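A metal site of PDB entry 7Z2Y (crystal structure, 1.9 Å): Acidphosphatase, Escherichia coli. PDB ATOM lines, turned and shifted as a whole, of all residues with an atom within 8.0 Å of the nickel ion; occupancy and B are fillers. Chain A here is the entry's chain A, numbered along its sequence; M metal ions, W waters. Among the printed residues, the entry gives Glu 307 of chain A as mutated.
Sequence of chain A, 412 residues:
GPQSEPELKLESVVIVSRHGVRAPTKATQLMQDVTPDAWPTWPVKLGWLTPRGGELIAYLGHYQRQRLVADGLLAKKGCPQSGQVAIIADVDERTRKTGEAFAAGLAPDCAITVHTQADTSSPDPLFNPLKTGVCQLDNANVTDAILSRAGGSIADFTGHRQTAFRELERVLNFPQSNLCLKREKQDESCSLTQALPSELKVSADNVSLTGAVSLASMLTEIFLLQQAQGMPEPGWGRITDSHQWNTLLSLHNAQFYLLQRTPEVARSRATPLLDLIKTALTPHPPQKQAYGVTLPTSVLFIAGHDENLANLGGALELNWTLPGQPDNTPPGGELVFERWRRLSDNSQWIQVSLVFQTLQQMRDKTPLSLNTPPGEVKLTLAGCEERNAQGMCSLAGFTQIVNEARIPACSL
OD2 of Asp 327 lies close to OE1 of Glu 221, at 2.7 Å. O of Thr 329 is in hydrogen-bond range of NH1 of Arg 18, at 2.9 Å. The guanidinium group (NH1) of Arg 18 is in salt-bridge range of the side-chain carboxylate (OD2) of Asp 327. The guanidinium group of Arg 18 is in salt-bridge range of the side-chain carboxylate of Asp 306, 2.9 Å away. N of Asp 327 lies close to OE1 of Gln 325 (3.1 Å). A ring nitrogen (ND1) of His 252 is in hydrogen-bond range of the side-chain hydroxyl (OG) of Ser 217 (3.2 Å).
The nickel ion is bound by water W1 (2.1 Å), the side-chain hydroxyl (OG1) of Thr 329 (2.1 Å), the side-chain carboxylate (OD1) of Asp 327 (2.2 Å) and a ring nitrogen (NE2) of His 252 (2.5 Å). The nickel ion has four donor atoms within binding distance.
Asp 306 touches the nickel ion (OD2 to NI, 3.6 Å). Of the 20 residues printed, 4 come within 4 Å of the nickel ion. Along chain A the residues within 4 Å of the nickel ion span positions 252 to 329.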
ATOM      1  N   ARG A  18      19.376  -3.550  13.378  1.00  0.00           N
ATOM      2  CA  ARG A  18      18.930  -2.222  13.760  1.00  0.00           C
ATOM      3  C   ARG A  18      18.693  -2.222  15.261  1.00  0.00           C
ATOM      4  O   ARG A  18      18.359  -3.246  15.857  1.00  0.00           O
ATOM      5  CB  ARG A  18      17.658  -1.836  13.003  1.00  0.00           C
ATOM      6  CG  ARG A  18      17.274  -0.377  13.155  1.00  0.00           C
ATOM      7  CD  ARG A  18      15.899  -0.104  12.570  1.00  0.00           C
ATOM      8  NE  ARG A  18      15.498   1.283  12.804  1.00  0.00           N
ATOM      9  CZ  ARG A  18      14.280   1.754  12.609  1.00  0.00           C
ATOM     10  NH1 ARG A  18      13.284   0.960  12.224  1.00  0.00           N
ATOM     11  NH2 ARG A  18      14.043   3.040  12.834  1.00  0.00           N
ATOM     12  N   SER A 217       7.749   9.650   5.577  1.00  0.00           N
ATOM     13  CA  SER A 217       8.599   8.566   6.041  1.00  0.00           C
ATOM     14  C   SER A 217       8.720   8.580   7.571  1.00  0.00           C
ATOM     15  O   SER A 217       8.677   7.518   8.216  1.00  0.00           O
ATOM     16  CB  SER A 217       9.976   8.674   5.391  1.00  0.00           C
ATOM     17  OG  SER A 217      10.801   7.605   5.780  1.00  0.00           O
ATOM     18  N   GLU A 221       6.750   5.800  10.365  1.00  0.00           N
ATOM     19  CA  GLU A 221       7.635   5.088  11.272  1.00  0.00           C
ATOM     20  C   GLU A 221       7.252   5.355  12.729  1.00  0.00           C
ATOM     21  O   GLU A 221       7.276   4.446  13.562  1.00  0.00           O
ATOM     22  CB  GLU A 221       9.083   5.508  11.018  1.00  0.00           C
ATOM     23  CG  GLU A 221      10.115   4.869  11.973  1.00  0.00           C
ATOM     24  CD  GLU A 221      10.328   3.396  11.723  1.00  0.00           C
ATOM     25  OE1 GLU A 221       9.674   2.818  10.799  1.00  0.00           O
ATOM     26  OE2 GLU A 221      11.160   2.810  12.429  1.00  0.00           O
ATOM     27  N   LEU A 224       4.449   3.211  13.597  1.00  0.00           N
ATOM     28  CA  LEU A 224       4.888   1.829  13.793  1.00  0.00           C
ATOM     29  C   LEU A 224       5.560   1.675  15.148  1.00  0.00           C
ATOM     30  O   LEU A 224       5.375   0.664  15.837  1.00  0.00           O
ATOM     31  CB  LEU A 224       5.857   1.405  12.675  1.00  0.00           C
ATOM     32  CG  LEU A 224       6.366  -0.032  12.794  1.00  0.00           C
ATOM     33  CD1 LEU A 224       5.646  -0.921  11.791  1.00  0.00           C
ATOM     34  CD2 LEU A 224       7.864  -0.099  12.583  1.00  0.00           C
ATOM     35  N   LEU A 249       3.323   2.437   5.895  1.00  0.00           N
ATOM     36  CA  LEU A 249       4.766   2.262   5.927  1.00  0.00           C
ATOM     37  C   LEU A 249       5.362   2.117   4.529  1.00  0.00           C
ATOM     38  O   LEU A 249       6.586   2.218   4.372  1.00  0.00           O
ATOM     39  CB  LEU A 249       5.069   1.043   6.799  1.00  0.00           C
ATOM     40  CG  LEU A 249       5.314   1.258   8.287  1.00  0.00           C
ATOM     41  CD1 LEU A 249       6.504   2.159   8.496  1.00  0.00           C
ATOM     42  CD2 LEU A 249       4.076   1.833   8.953  1.00  0.00           C
ATOM     43  N   HIS A 252       7.470   5.093   4.066  1.00  0.00           N
ATOM     44  CA  HIS A 252       8.761   4.968   4.731  1.00  0.00           C
ATOM     45  C   HIS A 252       9.705   4.087   3.915  1.00  0.00           C
ATOM     46  O   HIS A 252      10.859   4.448   3.684  1.00  0.00           O
ATOM     47  CB  HIS A 252       8.542   4.432   6.137  1.00  0.00           C
ATOM     48  CG  HIS A 252       9.797   4.080   6.856  1.00  0.00           C
ATOM     49  ND1 HIS A 252      10.523   5.000   7.585  1.00  0.00           N
ATOM     50  CD2 HIS A 252      10.462   2.911   6.967  1.00  0.00           C
ATOM     51  CE1 HIS A 252      11.577   4.405   8.111  1.00  0.00           C
ATOM     52  NE2 HIS A 252      11.567   3.140   7.753  1.00  0.00           N
ATOM     53  N   ASN A 253       9.202   2.946   3.441  1.00  0.00           N
ATOM     54  CA  ASN A 253      10.030   2.030   2.677  1.00  0.00           C
ATOM     55  C   ASN A 253      10.470   2.677   1.357  1.00  0.00           C
ATOM     56  O   ASN A 253      11.624   2.547   0.945  1.00  0.00           O
ATOM     57  CB  ASN A 253       9.258   0.728   2.446  1.00  0.00           C
ATOM     58  CG  ASN A 253       9.014  -0.053   3.752  1.00  0.00           C
ATOM     59  OD1 ASN A 253       9.808   0.042   4.709  1.00  0.00           O
ATOM     60  ND2 ASN A 253       7.904  -0.783   3.813  1.00  0.00           N
ATOM     61  N   PHE A 256      13.362   4.907   1.843  1.00  0.00           N
ATOM     62  CA  PHE A 256      14.615   4.179   2.017  1.00  0.00           C
ATOM     63  C   PHE A 256      15.055   3.518   0.718  1.00  0.00           C
ATOM     64  O   PHE A 256      16.248   3.389   0.463  1.00  0.00           O
ATOM     65  CB  PHE A 256      14.482   3.172   3.160  1.00  0.00           C
ATOM     66  CG  PHE A 256      14.880   3.749   4.480  1.00  0.00           C
ATOM     67  CD1 PHE A 256      13.992   4.553   5.194  1.00  0.00           C
ATOM     68  CD2 PHE A 256      16.124   3.473   5.036  1.00  0.00           C
ATOM     69  CE1 PHE A 256      14.375   5.118   6.408  1.00  0.00           C
ATOM     70  CE2 PHE A 256      16.505   4.021   6.267  1.00  0.00           C
ATOM     71  CZ  PHE A 256      15.631   4.830   6.948  1.00  0.00           C
ATOM     72  N   HIS A 305      21.757   0.854  12.450  1.00  0.00           N
ATOM     73  CA  HIS A 305      20.586   1.646  12.099  1.00  0.00           C
ATOM     74  C   HIS A 305      19.849   1.075  10.887  1.00  0.00           C
ATOM     75  O   HIS A 305      20.321   0.154  10.201  1.00  0.00           O
ATOM     76  CB  HIS A 305      20.998   3.108  11.817  1.00  0.00           C
ATOM     77  CG  HIS A 305      21.790   3.700  12.930  1.00  0.00           C
ATOM     78  ND1 HIS A 305      21.213   4.478  13.920  1.00  0.00           N
ATOM     79  CD2 HIS A 305      23.098   3.600  13.249  1.00  0.00           C
ATOM     80  CE1 HIS A 305      22.142   4.838  14.790  1.00  0.00           C
ATOM     81  NE2 HIS A 305      23.296   4.318  14.405  1.00  0.00           N
ATOM     82  N   ASP A 306      18.677   1.625  10.569  1.00  0.00           N
ATOM     83  CA  ASP A 306      18.005   1.056   9.410  1.00  0.00           C
ATOM     84  C   ASP A 306      18.688   1.491   8.105  1.00  0.00           C
ATOM     85  O   ASP A 306      18.670   0.722   7.129  1.00  0.00           O
ATOM     86  CB  ASP A 306      16.497   1.367   9.422  1.00  0.00           C
ATOM     87  CG  ASP A 306      16.188   2.815   9.678  1.00  0.00           C
ATOM     88  OD1 ASP A 306      17.029   3.694   9.427  1.00  0.00           O
ATOM     89  OD2 ASP A 306      15.045   3.076  10.104  1.00  0.00           O
ATOM     90  N   GLU A 307      19.331   2.655   8.079  1.00  0.00           N
ATOM     91  CA  GLU A 307      20.101   2.964   6.882  1.00  0.00           C
ATOM     92  C   GLU A 307      21.148   1.889   6.599  1.00  0.00           C
ATOM     93  O   GLU A 307      21.441   1.598   5.432  1.00  0.00           O
ATOM     94  CB  GLU A 307      20.815   4.294   7.017  1.00  0.00           C
ATOM     95  CG  GLU A 307      21.529   4.440   8.366  1.00  0.00           C
ATOM     96  CD  GLU A 307      22.576   5.562   8.397  1.00  0.00           C
ATOM     97  OE1 GLU A 307      22.345   6.599   7.731  1.00  0.00           O
ATOM     98  OE2 GLU A 307      23.565   5.469   9.166  1.00  0.00           O
ATOM     99  N   LEU A 309      21.064  -1.438   7.289  1.00  0.00           N
ATOM    100  CA  LEU A 309      20.423  -2.598   6.648  1.00  0.00           C
ATOM    101  C   LEU A 309      20.092  -2.292   5.196  1.00  0.00           C
ATOM    102  O   LEU A 309      20.315  -3.129   4.306  1.00  0.00           O
ATOM    103  CB  LEU A 309      19.157  -3.003   7.404  1.00  0.00           C
ATOM    104  CG  LEU A 309      19.288  -3.287   8.893  1.00  0.00           C
ATOM    105  CD1 LEU A 309      17.899  -3.414   9.418  1.00  0.00           C
ATOM    106  CD2 LEU A 309      20.054  -4.557   9.104  1.00  0.00           C
ATOM    107  N   ALA A 310      19.516  -1.109   4.952  1.00  0.00           N
ATOM    108  CA  ALA A 310      19.167  -0.729   3.587  1.00  0.00           C
ATOM    109  C   ALA A 310      20.423  -0.569   2.722  1.00  0.00           C
ATOM    110  O   ALA A 310      20.478  -1.049   1.574  1.00  0.00           O
ATOM    111  CB  ALA A 310      18.337   0.557   3.610  1.00  0.00           C
ATOM    112  N   GLN A 325       5.325  -7.537   8.724  1.00  0.00           N
ATOM    113  CA  GLN A 325       6.116  -6.457   9.322  1.00  0.00           C
ATOM    114  C   GLN A 325       6.160  -5.292   8.319  1.00  0.00           C
ATOM    115  O   GLN A 325       6.979  -5.315   7.385  1.00  0.00           O
ATOM    116  CB  GLN A 325       7.516  -6.959   9.688  1.00  0.00           C
ATOM    117  CG  GLN A 325       8.472  -5.873  10.156  1.00  0.00           C
ATOM    118  CD  GLN A 325       7.868  -4.992  11.231  1.00  0.00           C
ATOM    119  OE1 GLN A 325       7.433  -3.881  10.950  1.00  0.00           O
ATOM    120  NE2 GLN A 325       7.830  -5.496  12.467  1.00  0.00           N
ATOM    121  N   PRO A 326       5.291  -4.280   8.470  1.00  0.00           N
ATOM    122  CA  PRO A 326       5.208  -3.229   7.440  1.00  0.00           C
ATOM    123  C   PRO A 326       6.509  -2.500   7.201  1.00  0.00           C
ATOM    124  O   PRO A 326       6.708  -1.980   6.092  1.00  0.00           O
ATOM    125  CB  PRO A 326       4.120  -2.286   7.989  1.00  0.00           C
ATOM    126  CG  PRO A 326       3.332  -3.092   8.916  1.00  0.00           C
ATOM    127  CD  PRO A 326       4.316  -4.071   9.544  1.00  0.00           C
ATOM    128  N   ASP A 327       7.389  -2.426   8.179  1.00  0.00           N
ATOM    129  CA  ASP A 327       8.662  -1.712   8.030  1.00  0.00           C
ATOM    130  C   ASP A 327       9.728  -2.681   7.509  1.00  0.00           C
ATOM    131  O   ASP A 327      10.123  -3.608   8.221  1.00  0.00           O
ATOM    132  CB  ASP A 327       9.054  -1.090   9.364  1.00  0.00           C
ATOM    133  CG  ASP A 327      10.317  -0.276   9.281  1.00  0.00           C
ATOM    134  OD1 ASP A 327      10.946  -0.246   8.198  1.00  0.00           O
ATOM    135  OD2 ASP A 327      10.683   0.337  10.309  1.00  0.00           O
ATOM    136  N   ASN A 328      10.202  -2.465   6.261  1.00  0.00           N
ATOM    137  CA  ASN A 328      11.200  -3.349   5.652  1.00  0.00           C
ATOM    138  C   ASN A 328      12.511  -3.380   6.424  1.00  0.00           C
ATOM    139  O   ASN A 328      13.334  -4.288   6.212  1.00  0.00           O
ATOM    140  CB  ASN A 328      11.600  -2.899   4.243  1.00  0.00           C
ATOM    141  CG  ASN A 328      10.567  -3.246   3.221  1.00  0.00           C
ATOM    142  OD1 ASN A 328       9.678  -4.040   3.496  1.00  0.00           O
ATOM    143  ND2 ASN A 328      10.707  -2.689   2.001  1.00  0.00           N
ATOM    144  N   THR A 329      12.782  -2.364   7.251  1.00  0.00           N
ATOM    145  CA  THR A 329      13.996  -2.299   8.066  1.00  0.00           C
ATOM    146  C   THR A 329      13.558  -1.998   9.491  1.00  0.00           C
ATOM    147  O   THR A 329      13.806  -0.897  10.007  1.00  0.00           O
ATOM    148  CB  THR A 329      14.982  -1.261   7.522  1.00  0.00           C
ATOM    149  OG1 THR A 329      14.298  -0.055   7.186  1.00  0.00           O
ATOM    150  CG2 THR A 329      15.616  -1.782   6.229  1.00  0.00           C
ATOM    151  N   PRO A 330      12.899  -2.953  10.149  1.00  0.00           N
ATOM    152  CA  PRO A 330      12.216  -2.655  11.406  1.00  0.00           C
ATOM    153  C   PRO A 330      13.166  -2.638  12.604  1.00  0.00           C
ATOM    154  O   PRO A 330      14.278  -3.174  12.547  1.00  0.00           O
ATOM    155  CB  PRO A 330      11.213  -3.816  11.529  1.00  0.00           C
ATOM    156  CG  PRO A 330      11.924  -4.946  10.899  1.00  0.00           C
ATOM    157  CD  PRO A 330      12.764  -4.365   9.777  1.00  0.00           C
ATOM    158  N   PRO A 331      12.715  -2.044  13.710  1.00  0.00           N
ATOM    159  CA  PRO A 331      13.475  -2.111  14.968  1.00  0.00           C
ATOM    160  C   PRO A 331      13.836  -3.544  15.314  1.00  0.00           C
ATOM    161  O   PRO A 331      12.992  -4.434  15.295  1.00  0.00           O
ATOM    162  CB  PRO A 331      12.493  -1.537  16.000  1.00  0.00           C
ATOM    163  CG  PRO A 331      11.613  -0.662  15.202  1.00  0.00           C
ATOM    164  CD  PRO A 331      11.467  -1.290  13.854  1.00  0.00           C
HETATM  165 NI    NI M   1      12.775   1.035   8.143  1.00  0.00          NI
HETATM  166  O   HOH W   1      13.025   2.027   9.959  1.00  0.00           O
HETATM  167  O   HOH W   2      12.716   0.838   5.193  1.00  0.00           O
